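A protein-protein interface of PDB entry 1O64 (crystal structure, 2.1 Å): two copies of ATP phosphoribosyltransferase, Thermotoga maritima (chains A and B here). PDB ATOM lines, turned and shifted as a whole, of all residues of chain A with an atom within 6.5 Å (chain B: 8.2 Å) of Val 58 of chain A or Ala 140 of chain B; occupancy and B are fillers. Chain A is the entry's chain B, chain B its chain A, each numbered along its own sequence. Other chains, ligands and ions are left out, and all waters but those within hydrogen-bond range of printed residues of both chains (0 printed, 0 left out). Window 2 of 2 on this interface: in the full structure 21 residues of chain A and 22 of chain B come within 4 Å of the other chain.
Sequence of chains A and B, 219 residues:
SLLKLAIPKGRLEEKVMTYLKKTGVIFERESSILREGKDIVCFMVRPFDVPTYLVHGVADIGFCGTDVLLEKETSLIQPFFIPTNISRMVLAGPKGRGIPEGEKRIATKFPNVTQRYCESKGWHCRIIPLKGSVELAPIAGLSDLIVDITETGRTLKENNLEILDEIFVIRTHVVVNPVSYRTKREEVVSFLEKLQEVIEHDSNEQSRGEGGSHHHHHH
N of Ala 137 of chain B lies within hydrogen-bond range of OH of Tyr 53 of chain A, at 3.5 Å.
The backbone carbonyl oxygen (O) of Leu 142 of chain B sits at hydrogen-bond distance from the guanidinium group (NH2) of Arg 105 of chain B, 3.2 Å away. O of Tyr 53 of chain A is in hydrogen-bond range of N of Ala 59 of chain A (2.8 Å). The backbone NH (N) of Leu 142 of chain B is in hydrogen-bond range of the backbone carbonyl oxygen (O) of Ala 137 of chain B, 3.0 Å away. The backbone carbonyl oxygen (O) of Leu 5 of chain A lies within hydrogen-bond range of the backbone NH (N) of Phe 43 of chain A (2.6 Å). O of Ala 137 of chain B is in hydrogen-bond range of N of Ser 143 of chain B (3.5 Å).
Among the printed residues, pairs that only touch across the chains: Phe 43 of chain A with Leu 136 of chain B, Phe 43 of chain A with Ala 140 of chain B, Thr 52 of chain A with Ile 128 of chain B, Tyr 53 of chain A with Leu 136 of chain B, Tyr 53 of chain A with Ala 140 of chain B, Tyr 53 of chain A with Leu 142 of chain B and Val 58 of chain A with Ala 140 of chain B.
Val 58 of chain A touches one residue of chain B. Ala 140 of chain B touches just these residues of chain A: Phe 43 (3.6 Å), Tyr 53 (3.6 Å) and Val 58 (3.7 Å). No residue of chain B comes within 4 Å of Ala 59 of chain A. Of the printed residues of chain A, Leu 136 of chain B touches Phe 43 (3.7 Å) and Tyr 53 (3.7 Å). Printed residues of chain A within 4 Å of Leu 142 of chain B: Tyr 53. Of the printed residues of chain B, Tyr 53 of chain A touches Leu 136, Ala 137, Ala 140 and Leu 142. Of the printed residues of chain B, Phe 43 of chain A touches Leu 136 and Ala 140. The nearest printed residue of chain B that does not touch Thr 52 of chain A is Leu 142 of chain B (4.02 Å).
Of the 12 printed residues of chain B, 5 touch a printed residue of chain A. Printed residues of chain B that touch a printed residue of chain A: Ile 128, Leu 136, Ala 137, Ala 140 and Leu 142. Hydrophobic or aromatic side chains of chain B within 4 Å of the printed part of chain A: Ile 128, Leu 136, Ala 140 and Leu 142. Among the printed residues, no Asp or Glu carboxylate lies within 4 Å of a Lys or Arg side-chain nitrogen of the other chain.
No position is printed for both chains. Of the 8 pairs that touch across the chains among the printed residues, none has its exchanged pair printed and touching as well.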
ATOM      1  N   LYS A   4     -28.662  17.169  21.375  1.00  0.00           N
ATOM      2  CA  LYS A   4     -27.795  18.257  20.905  1.00  0.00           C
ATOM      3  C   LYS A   4     -27.222  19.007  22.100  1.00  0.00           C
ATOM      4  O   LYS A   4     -27.973  19.402  23.000  1.00  0.00           O
ATOM      5  CB  LYS A   4     -28.594  19.199  20.002  1.00  0.00           C
ATOM      6  CG  LYS A   4     -28.843  18.513  18.644  1.00  0.00           C
ATOM      7  CD  LYS A   4     -30.191  18.843  18.072  1.00  0.00           C
ATOM      8  CE  LYS A   4     -30.846  17.625  17.469  1.00  0.00           C
ATOM      9  NZ  LYS A   4     -29.859  16.655  16.904  1.00  0.00           N
ATOM     10  N   LEU A   5     -25.908  19.102  22.138  1.00  0.00           N
ATOM     11  CA  LEU A   5     -25.206  19.762  23.232  1.00  0.00           C
ATOM     12  C   LEU A   5     -24.604  21.105  22.809  1.00  0.00           C
ATOM     13  O   LEU A   5     -24.061  21.207  21.709  1.00  0.00           O
ATOM     14  CB  LEU A   5     -24.075  18.843  23.702  1.00  0.00           C
ATOM     15  CG  LEU A   5     -24.330  17.719  24.673  1.00  0.00           C
ATOM     16  CD1 LEU A   5     -25.509  16.869  24.351  1.00  0.00           C
ATOM     17  CD2 LEU A   5     -23.063  16.828  24.798  1.00  0.00           C
ATOM     18  N   PHE A  43     -22.607  21.605  19.532  1.00  0.00           N
ATOM     19  CA  PHE A  43     -22.425  22.938  18.926  1.00  0.00           C
ATOM     20  C   PHE A  43     -21.389  23.674  19.791  1.00  0.00           C
ATOM     21  O   PHE A  43     -21.622  23.851  20.988  1.00  0.00           O
ATOM     22  CB  PHE A  43     -23.736  23.684  18.843  1.00  0.00           C
ATOM     23  CG  PHE A  43     -24.845  22.974  18.130  1.00  0.00           C
ATOM     24  CD1 PHE A  43     -26.067  22.749  18.751  1.00  0.00           C
ATOM     25  CD2 PHE A  43     -24.683  22.571  16.813  1.00  0.00           C
ATOM     26  CE1 PHE A  43     -27.085  22.108  18.061  1.00  0.00           C
ATOM     27  CE2 PHE A  43     -25.697  21.934  16.116  1.00  0.00           C
ATOM     28  CZ  PHE A  43     -26.893  21.698  16.751  1.00  0.00           C
ATOM     29  N   THR A  52     -28.566  30.806  24.933  1.00  0.00           N
ATOM     30  CA  THR A  52     -29.327  31.163  23.742  1.00  0.00           C
ATOM     31  C   THR A  52     -29.534  30.006  22.800  1.00  0.00           C
ATOM     32  O   THR A  52     -30.601  29.976  22.133  1.00  0.00           O
ATOM     33  CB  THR A  52     -28.939  32.500  23.128  1.00  0.00           C
ATOM     34  OG1 THR A  52     -28.618  32.503  21.746  1.00  0.00           O
ATOM     35  CG2 THR A  52     -27.885  33.216  23.913  1.00  0.00           C
ATOM     36  N   TYR A  53     -28.703  28.970  22.834  1.00  0.00           N
ATOM     37  CA  TYR A  53     -28.931  27.770  22.048  1.00  0.00           C
ATOM     38  C   TYR A  53     -29.847  26.781  22.773  1.00  0.00           C
ATOM     39  O   TYR A  53     -30.334  25.809  22.164  1.00  0.00           O
ATOM     40  CB  TYR A  53     -27.623  27.043  21.704  1.00  0.00           C
ATOM     41  CG  TYR A  53     -26.939  27.545  20.450  1.00  0.00           C
ATOM     42  CD1 TYR A  53     -26.188  28.718  20.469  1.00  0.00           C
ATOM     43  CD2 TYR A  53     -27.027  26.853  19.251  1.00  0.00           C
ATOM     44  CE1 TYR A  53     -25.563  29.190  19.332  1.00  0.00           C
ATOM     45  CE2 TYR A  53     -26.393  27.309  18.109  1.00  0.00           C
ATOM     46  CZ  TYR A  53     -25.679  28.482  18.147  1.00  0.00           C
ATOM     47  OH  TYR A  53     -25.054  28.955  16.998  1.00  0.00           O
ATOM     48  N   LEU A  54     -30.075  26.914  24.077  1.00  0.00           N
ATOM     49  CA  LEU A  54     -30.926  25.942  24.777  1.00  0.00           C
ATOM     50  C   LEU A  54     -32.386  26.359  24.807  1.00  0.00           C
ATOM     51  O   LEU A  54     -33.016  26.479  25.862  1.00  0.00           O
ATOM     52  CB  LEU A  54     -30.371  25.744  26.205  1.00  0.00           C
ATOM     53  CG  LEU A  54     -28.952  25.151  26.245  1.00  0.00           C
ATOM     54  CD1 LEU A  54     -28.308  25.372  27.621  1.00  0.00           C
ATOM     55  CD2 LEU A  54     -29.000  23.679  25.895  1.00  0.00           C
ATOM     56  N   VAL A  55     -32.971  26.643  23.656  1.00  0.00           N
ATOM     57  CA  VAL A  55     -34.330  27.108  23.504  1.00  0.00           C
ATOM     58  C   VAL A  55     -35.086  26.273  22.463  1.00  0.00           C
ATOM     59  O   VAL A  55     -34.478  25.612  21.630  1.00  0.00           O
ATOM     60  CB  VAL A  55     -34.437  28.579  23.038  1.00  0.00           C
ATOM     61  CG1 VAL A  55     -33.692  29.518  23.970  1.00  0.00           C
ATOM     62  CG2 VAL A  55     -33.971  28.708  21.599  1.00  0.00           C
ATOM     63  N   HIS A  56     -36.421  26.346  22.582  1.00  0.00           N
ATOM     64  CA  HIS A  56     -37.281  25.608  21.653  1.00  0.00           C
ATOM     65  C   HIS A  56     -36.677  24.268  21.296  1.00  0.00           C
ATOM     66  O   HIS A  56     -36.323  23.468  22.190  1.00  0.00           O
ATOM     67  CB  HIS A  56     -37.600  26.447  20.411  1.00  0.00           C
ATOM     68  CG  HIS A  56     -37.933  27.872  20.749  1.00  0.00           C
ATOM     69  ND1 HIS A  56     -39.068  28.222  21.460  1.00  0.00           N
ATOM     70  CD2 HIS A  56     -37.255  29.022  20.510  1.00  0.00           C
ATOM     71  CE1 HIS A  56     -39.081  29.537  21.631  1.00  0.00           C
ATOM     72  NE2 HIS A  56     -37.991  30.040  21.073  1.00  0.00           N
ATOM     73  N   GLY A  57     -36.544  23.970  20.013  1.00  0.00           N
ATOM     74  CA  GLY A  57     -35.930  22.706  19.606  1.00  0.00           C
ATOM     75  C   GLY A  57     -34.511  22.860  19.086  1.00  0.00           C
ATOM     76  O   GLY A  57     -34.147  22.076  18.185  1.00  0.00           O
ATOM     77  N   VAL A  58     -33.662  23.758  19.612  1.00  0.00           N
ATOM     78  CA  VAL A  58     -32.296  23.823  19.043  1.00  0.00           C
ATOM     79  C   VAL A  58     -31.307  23.012  19.826  1.00  0.00           C
ATOM     80  O   VAL A  58     -30.727  22.048  19.256  1.00  0.00           O
ATOM     81  CB  VAL A  58     -31.847  25.190  18.559  1.00  0.00           C
ATOM     82  CG1 VAL A  58     -32.772  26.326  18.970  1.00  0.00           C
ATOM     83  CG2 VAL A  58     -30.393  25.548  18.846  1.00  0.00           C
ATOM     84  N   ALA A  59     -31.026  23.291  21.103  1.00  0.00           N
ATOM     85  CA  ALA A  59     -30.116  22.374  21.825  1.00  0.00           C
ATOM     86  C   ALA A  59     -30.807  21.795  23.053  1.00  0.00           C
ATOM     87  O   ALA A  59     -31.743  22.408  23.562  1.00  0.00           O
ATOM     88  CB  ALA A  59     -28.812  23.062  22.170  1.00  0.00           C
ATOM     89  N   ASP A  60     -30.341  20.665  23.563  1.00  0.00           N
ATOM     90  CA  ASP A  60     -30.959  20.004  24.701  1.00  0.00           C
ATOM     91  C   ASP A  60     -30.231  20.200  26.022  1.00  0.00           C
ATOM     92  O   ASP A  60     -30.880  20.356  27.061  1.00  0.00           O
ATOM     93  CB  ASP A  60     -30.998  18.472  24.427  1.00  0.00           C
ATOM     94  CG  ASP A  60     -31.763  18.173  23.132  1.00  0.00           C
ATOM     95  OD1 ASP A  60     -32.919  18.654  23.005  1.00  0.00           O
ATOM     96  OD2 ASP A  60     -31.235  17.461  22.274  1.00  0.00           O
ATOM     97  N   ASN A 177     -32.383  22.436  28.546  1.00  0.00           N
ATOM     98  CA  ASN A 177     -33.529  23.136  27.944  1.00  0.00           C
ATOM     99  C   ASN A 177     -34.807  22.479  28.482  1.00  0.00           C
ATOM    100  O   ASN A 177     -34.932  21.258  28.420  1.00  0.00           O
ATOM    101  CB  ASN A 177     -33.444  22.955  26.422  1.00  0.00           C
ATOM    102  CG  ASN A 177     -34.576  23.582  25.651  1.00  0.00           C
ATOM    103  OD1 ASN A 177     -35.500  24.175  26.206  1.00  0.00           O
ATOM    104  ND2 ASN A 177     -34.528  23.492  24.325  1.00  0.00           N
ATOM    105  N   SER A 180     -36.713  20.318  26.050  1.00  0.00           N
ATOM    106  CA  SER A 180     -36.067  19.026  25.877  1.00  0.00           C
ATOM    107  C   SER A 180     -36.296  18.082  27.032  1.00  0.00           C
ATOM    108  O   SER A 180     -36.465  16.865  26.860  1.00  0.00           O
ATOM    109  CB  SER A 180     -34.550  19.163  25.639  1.00  0.00           C
ATOM    110  OG  SER A 180     -34.330  19.997  24.526  1.00  0.00           O
ATOM    111  N   ARG B 105     -35.730  34.737  10.859  1.00  0.00           N
ATOM    112  CA  ARG B 105     -34.933  34.596  12.090  1.00  0.00           C
ATOM    113  C   ARG B 105     -33.470  34.882  11.728  1.00  0.00           C
ATOM    114  O   ARG B 105     -32.893  34.199  10.895  1.00  0.00           O
ATOM    115  CB  ARG B 105     -35.091  33.211  12.691  1.00  0.00           C
ATOM    116  CG  ARG B 105     -36.351  33.040  13.549  1.00  0.00           C
ATOM    117  CD  ARG B 105     -36.451  31.591  14.034  1.00  0.00           C
ATOM    118  NE  ARG B 105     -36.229  30.686  12.910  1.00  0.00           N
ATOM    119  CZ  ARG B 105     -35.640  29.508  12.991  1.00  0.00           C
ATOM    120  NH1 ARG B 105     -35.470  28.784  11.888  1.00  0.00           N
ATOM    121  NH2 ARG B 105     -35.229  29.036  14.156  1.00  0.00           N
ATOM    122  N   ILE B 128     -31.626  37.364  16.839  1.00  0.00           N
ATOM    123  CA  ILE B 128     -30.976  36.606  17.921  1.00  0.00           C
ATOM    124  C   ILE B 128     -29.524  37.036  18.063  1.00  0.00           C
ATOM    125  O   ILE B 128     -28.696  36.678  17.227  1.00  0.00           O
ATOM    126  CB  ILE B 128     -31.025  35.106  17.585  1.00  0.00           C
ATOM    127  CG1 ILE B 128     -32.475  34.655  17.364  1.00  0.00           C
ATOM    128  CG2 ILE B 128     -30.369  34.264  18.666  1.00  0.00           C
ATOM    129  CD1 ILE B 128     -32.615  33.655  16.229  1.00  0.00           C
ATOM    130  N   VAL B 134     -21.126  32.982  14.503  1.00  0.00           N
ATOM    131  CA  VAL B 134     -22.482  33.203  14.058  1.00  0.00           C
ATOM    132  C   VAL B 134     -22.848  32.286  12.905  1.00  0.00           C
ATOM    133  O   VAL B 134     -24.016  31.962  12.724  1.00  0.00           O
ATOM    134  CB  VAL B 134     -22.713  34.681  13.642  1.00  0.00           C
ATOM    135  CG1 VAL B 134     -24.179  34.942  13.343  1.00  0.00           C
ATOM    136  CG2 VAL B 134     -22.271  35.603  14.784  1.00  0.00           C
ATOM    137  N   GLU B 135     -21.890  31.817  12.127  1.00  0.00           N
ATOM    138  CA  GLU B 135     -22.122  30.924  11.012  1.00  0.00           C
ATOM    139  C   GLU B 135     -22.678  29.566  11.437  1.00  0.00           C
ATOM    140  O   GLU B 135     -23.129  28.810  10.582  1.00  0.00           O
ATOM    141  CB  GLU B 135     -20.828  30.731  10.197  1.00  0.00           C
ATOM    142  CG  GLU B 135     -19.795  29.896  10.946  1.00  0.00           C
ATOM    143  CD  GLU B 135     -18.888  30.761  11.802  1.00  0.00           C
ATOM    144  OE1 GLU B 135     -19.111  31.991  11.867  1.00  0.00           O
ATOM    145  OE2 GLU B 135     -17.942  30.219  12.412  1.00  0.00           O
ATOM    146  N   LEU B 136     -22.667  29.227  12.715  1.00  0.00           N
ATOM    147  CA  LEU B 136     -23.203  27.979  13.230  1.00  0.00           C
ATOM    148  C   LEU B 136     -24.719  28.050  13.404  1.00  0.00           C
ATOM    149  O   LEU B 136     -25.359  26.997  13.394  1.00  0.00           O
ATOM    150  CB  LEU B 136     -22.582  27.637  14.584  1.00  0.00           C
ATOM    151  CG  LEU B 136     -23.008  26.336  15.263  1.00  0.00           C
ATOM    152  CD1 LEU B 136     -22.771  25.124  14.370  1.00  0.00           C
ATOM    153  CD2 LEU B 136     -22.261  26.167  16.583  1.00  0.00           C
ATOM    154  N   ALA B 137     -25.277  29.255  13.520  1.00  0.00           N
ATOM    155  CA  ALA B 137     -26.692  29.430  13.738  1.00  0.00           C
ATOM    156  C   ALA B 137     -27.632  28.707  12.785  1.00  0.00           C
ATOM    157  O   ALA B 137     -28.544  28.044  13.265  1.00  0.00           O
ATOM    158  CB  ALA B 137     -27.060  30.913  13.831  1.00  0.00           C
ATOM    159  N   PRO B 138     -27.481  28.814  11.481  1.00  0.00           N
ATOM    160  CA  PRO B 138     -28.372  28.193  10.518  1.00  0.00           C
ATOM    161  C   PRO B 138     -28.325  26.675  10.566  1.00  0.00           C
ATOM    162  O   PRO B 138     -29.373  26.031  10.698  1.00  0.00           O
ATOM    163  CB  PRO B 138     -27.915  28.708   9.165  1.00  0.00           C
ATOM    164  CG  PRO B 138     -27.163  29.973   9.471  1.00  0.00           C
ATOM    165  CD  PRO B 138     -26.511  29.726  10.811  1.00  0.00           C
ATOM    166  N   ILE B 139     -27.121  26.105  10.620  1.00  0.00           N
ATOM    167  CA  ILE B 139     -26.969  24.659  10.687  1.00  0.00           C
ATOM    168  C   ILE B 139     -27.532  24.080  11.968  1.00  0.00           C
ATOM    169  O   ILE B 139     -28.046  22.949  11.962  1.00  0.00           O
ATOM    170  CB  ILE B 139     -25.515  24.223  10.444  1.00  0.00           C
ATOM    171  CG1 ILE B 139     -25.494  22.875   9.700  1.00  0.00           C
ATOM    172  CG2 ILE B 139     -24.699  24.147  11.716  1.00  0.00           C
ATOM    173  CD1 ILE B 139     -25.786  23.021   8.211  1.00  0.00           C
ATOM    174  N   ALA B 140     -27.532  24.821  13.068  1.00  0.00           N
ATOM    175  CA  ALA B 140     -28.080  24.349  14.332  1.00  0.00           C
ATOM    176  C   ALA B 140     -29.594  24.567  14.407  1.00  0.00           C
ATOM    177  O   ALA B 140     -30.235  24.153  15.361  1.00  0.00           O
ATOM    178  CB  ALA B 140     -27.399  25.075  15.500  1.00  0.00           C
ATOM    179  N   GLY B 141     -30.193  25.271  13.450  1.00  0.00           N
ATOM    180  CA  GLY B 141     -31.624  25.552  13.486  1.00  0.00           C
ATOM    181  C   GLY B 141     -32.002  26.751  14.345  1.00  0.00           C
ATOM    182  O   GLY B 141     -33.187  27.017  14.583  1.00  0.00           O
ATOM    183  N   LEU B 142     -31.012  27.495  14.854  1.00  0.00           N
ATOM    184  CA  LEU B 142     -31.266  28.658  15.702  1.00  0.00           C
ATOM    185  C   LEU B 142     -31.874  29.801  14.878  1.00  0.00           C
ATOM    186  O   LEU B 142     -32.674  30.615  15.349  1.00  0.00           O
ATOM    187  CB  LEU B 142     -29.942  29.143  16.306  1.00  0.00           C
ATOM    188  CG  LEU B 142     -29.877  29.749  17.683  1.00  0.00           C
ATOM    189  CD1 LEU B 142     -28.713  30.744  17.826  1.00  0.00           C
ATOM    190  CD2 LEU B 142     -31.170  30.342  18.168  1.00  0.00           C
ATOM    191  N   SER B 143     -31.393  29.953  13.652  1.00  0.00           N
ATOM    192  CA  SER B 143     -31.905  31.018  12.790  1.00  0.00           C
ATOM    193  C   SER B 143     -31.962  30.532  11.345  1.00  0.00           C
ATOM    194  O   SER B 143     -31.324  29.526  11.027  1.00  0.00           O
ATOM    195  CB  SER B 143     -30.968  32.256  12.824  1.00  0.00           C
ATOM    196  OG  SER B 143     -29.781  31.968  12.078  1.00  0.00           O
